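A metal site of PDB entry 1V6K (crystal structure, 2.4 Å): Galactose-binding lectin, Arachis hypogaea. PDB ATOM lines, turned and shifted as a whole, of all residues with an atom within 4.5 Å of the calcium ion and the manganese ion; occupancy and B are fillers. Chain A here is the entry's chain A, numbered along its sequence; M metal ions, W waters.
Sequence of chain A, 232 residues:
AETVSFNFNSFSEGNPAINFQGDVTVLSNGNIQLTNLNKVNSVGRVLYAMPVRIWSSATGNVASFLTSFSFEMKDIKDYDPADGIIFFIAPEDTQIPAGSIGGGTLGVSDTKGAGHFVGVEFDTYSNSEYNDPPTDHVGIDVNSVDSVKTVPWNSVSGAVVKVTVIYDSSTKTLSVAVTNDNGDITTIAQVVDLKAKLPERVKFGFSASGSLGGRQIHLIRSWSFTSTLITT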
ATOM      1  N   GLY A 104      -2.454 -26.329  21.007  1.00  0.00           N
ATOM      2  CA  GLY A 104      -2.369 -26.537  19.569  1.00  0.00           C
ATOM      3  C   GLY A 104      -3.314 -27.562  18.973  1.00  0.00           C
ATOM      4  O   GLY A 104      -3.358 -27.703  17.749  1.00  0.00           O
ATOM      5  N   GLU A 121      -8.257 -23.583   9.794  1.00  0.00           N
ATOM      6  CA  GLU A 121      -7.742 -22.992  11.016  1.00  0.00           C
ATOM      7  C   GLU A 121      -7.125 -21.613  10.842  1.00  0.00           C
ATOM      8  O   GLU A 121      -6.607 -21.260   9.778  1.00  0.00           O
ATOM      9  CB  GLU A 121      -6.718 -23.923  11.653  1.00  0.00           C
ATOM     10  CG  GLU A 121      -5.565 -24.265  10.737  1.00  0.00           C
ATOM     11  CD  GLU A 121      -4.469 -24.968  11.457  1.00  0.00           C
ATOM     12  OE1 GLU A 121      -4.719 -26.030  12.059  1.00  0.00           O
ATOM     13  OE2 GLU A 121      -3.336 -24.461  11.433  1.00  0.00           O
ATOM     14  N   ASP A 123      -4.605 -20.187  12.964  1.00  0.00           N
ATOM     15  CA  ASP A 123      -3.599 -20.505  13.941  1.00  0.00           C
ATOM     16  C   ASP A 123      -2.689 -19.361  14.316  1.00  0.00           C
ATOM     17  O   ASP A 123      -2.037 -18.787  13.458  1.00  0.00           O
ATOM     18  CB  ASP A 123      -2.768 -21.650  13.397  1.00  0.00           C
ATOM     19  CG  ASP A 123      -2.260 -22.529  14.474  1.00  0.00           C
ATOM     20  OD1 ASP A 123      -1.880 -21.990  15.538  1.00  0.00           O
ATOM     21  OD2 ASP A 123      -2.238 -23.752  14.263  1.00  0.00           O
ATOM     22  N   TYR A 125      -0.285 -19.624  17.014  1.00  0.00           N
ATOM     23  CA  TYR A 125       0.879 -20.072  17.760  1.00  0.00           C
ATOM     24  C   TYR A 125       1.539 -21.214  17.009  1.00  0.00           C
ATOM     25  O   TYR A 125       0.866 -22.104  16.511  1.00  0.00           O
ATOM     26  CB  TYR A 125       0.506 -20.531  19.164  1.00  0.00           C
ATOM     27  CG  TYR A 125       1.716 -20.970  19.950  1.00  0.00           C
ATOM     28  CD1 TYR A 125       2.199 -22.272  19.858  1.00  0.00           C
ATOM     29  CD2 TYR A 125       2.419 -20.051  20.741  1.00  0.00           C
ATOM     30  CE1 TYR A 125       3.365 -22.658  20.525  1.00  0.00           C
ATOM     31  CE2 TYR A 125       3.580 -20.426  21.417  1.00  0.00           C
ATOM     32  CZ  TYR A 125       4.046 -21.732  21.307  1.00  0.00           C
ATOM     33  OH  TYR A 125       5.180 -22.114  21.974  1.00  0.00           O
ATOM     34  N   ASN A 127       3.094 -24.508  16.824  1.00  0.00           N
ATOM     35  CA  ASN A 127       3.319 -25.769  17.516  1.00  0.00           C
ATOM     36  C   ASN A 127       4.200 -26.637  16.632  1.00  0.00           C
ATOM     37  O   ASN A 127       3.724 -27.184  15.635  1.00  0.00           O
ATOM     38  CB  ASN A 127       2.012 -26.517  17.766  1.00  0.00           C
ATOM     39  CG  ASN A 127       1.176 -25.871  18.845  1.00  0.00           C
ATOM     40  OD1 ASN A 127       0.568 -24.837  18.619  1.00  0.00           O
ATOM     41  ND2 ASN A 127       1.156 -26.475  20.036  1.00  0.00           N
ATOM     42  N   ASP A 132       3.819 -26.778  12.477  1.00  0.00           N
ATOM     43  CA  ASP A 132       3.279 -25.475  12.124  1.00  0.00           C
ATOM     44  C   ASP A 132       4.307 -24.586  11.474  1.00  0.00           C
ATOM     45  O   ASP A 132       5.496 -24.663  11.786  1.00  0.00           O
ATOM     46  CB  ASP A 132       2.782 -24.722  13.349  1.00  0.00           C
ATOM     47  CG  ASP A 132       1.441 -25.174  13.818  1.00  0.00           C
ATOM     48  OD1 ASP A 132       0.604 -25.561  12.978  1.00  0.00           O
ATOM     49  OD2 ASP A 132       1.211 -25.124  15.040  1.00  0.00           O
ATOM     50  N   HIS A 137      -0.902 -18.354  10.738  1.00  0.00           N
ATOM     51  CA  HIS A 137      -1.267 -18.868   9.438  1.00  0.00           C
ATOM     52  C   HIS A 137      -2.685 -19.396   9.320  1.00  0.00           C
ATOM     53  O   HIS A 137      -3.371 -19.627  10.318  1.00  0.00           O
ATOM     54  CB  HIS A 137      -0.315 -19.992   9.076  1.00  0.00           C
ATOM     55  CG  HIS A 137      -0.276 -21.086  10.087  1.00  0.00           C
ATOM     56  ND1 HIS A 137       0.412 -20.963  11.284  1.00  0.00           N
ATOM     57  CD2 HIS A 137      -0.893 -22.285  10.128  1.00  0.00           C
ATOM     58  CE1 HIS A 137       0.219 -22.045  12.010  1.00  0.00           C
ATOM     59  NE2 HIS A 137      -0.573 -22.866  11.331  1.00  0.00           N
ATOM     60  N   VAL A 145      -4.249 -31.640  12.815  1.00  0.00           N
ATOM     61  CA  VAL A 145      -3.920 -30.236  12.981  1.00  0.00           C
ATOM     62  C   VAL A 145      -2.582 -29.969  12.298  1.00  0.00           C
ATOM     63  O   VAL A 145      -2.068 -28.850  12.310  1.00  0.00           O
ATOM     64  CB  VAL A 145      -3.845 -29.834  14.466  1.00  0.00           C
ATOM     65  CG1 VAL A 145      -5.209 -29.953  15.094  1.00  0.00           C
ATOM     66  CG2 VAL A 145      -2.824 -30.684  15.193  1.00  0.00           C
ATOM     67  N   SER A 147      -1.538 -29.381   9.248  1.00  0.00           N
ATOM     68  CA  SER A 147      -2.116 -28.947   7.980  1.00  0.00           C
ATOM     69  C   SER A 147      -1.607 -29.558   6.683  1.00  0.00           C
ATOM     70  O   SER A 147      -0.407 -29.761   6.480  1.00  0.00           O
ATOM     71  CB  SER A 147      -2.028 -27.422   7.880  1.00  0.00           C
ATOM     72  OG  SER A 147      -2.789 -26.805   8.911  1.00  0.00           O
HETATM   73 CA    CA M   1      -0.649 -24.119  16.444  1.00  0.00          CA
HETATM   74 MN    MN M   2      -1.351 -24.639  12.481  1.00  0.00          MN
HETATM   75  O   HOH W   1      -0.954 -25.694  10.523  1.00  0.00           O
HETATM   76  O   HOH W   2      -2.378 -26.600  13.308  1.00  0.00           O
HETATM   77  O   HOH W   3      -2.339 -23.228  18.334  1.00  0.00           O
HETATM   78  O   HOH W   4      -1.929 -26.345  16.008  1.00  0.00           O
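The side-chain carboxylate (OE2) of Glu 121 lies close to the side-chain hydroxyl (OG) of Ser 147, at 3.5 Å.
The nearest printed residue that does not touch the calcium ion is Gly 104 (4.3 Å).
Of the 9 residues printed, 4 come within 4 Å of the manganese ion.
Along chain A the residues within 4 Å of the manganese ion span positions 121 to 137.
The nearest printed residue that does not touch the manganese ion is Val 145 (4.3 Å).
The calcium ion is bound by O of Tyr 125 (2.5 Å), OD2 of Asp 132 (2.5 Å), OD1 of Asn 127 (2.6 Å), water W4 (2.6 Å), OD1 of Asp 123 (2.6 Å), water W3 (2.7 Å) and OD2 of Asp 123 (2.7 Å).
The calcium ion has seven donor atoms within binding distance.
The manganese ion is bound by OD2 of Asp 123 (2.2 Å), OD1 of Asp 132 (2.2 Å), OE2 of Glu 121 (2.3 Å), NE2 of His 137 (2.3 Å), water W1 (2.3 Å) and water W2 (2.4 Å).
The manganese ion has six donor atoms within binding distance.
Water W2 bridges O of Val 145 (2.5 Å) and OE1 of Glu 121 (2.7 Å).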
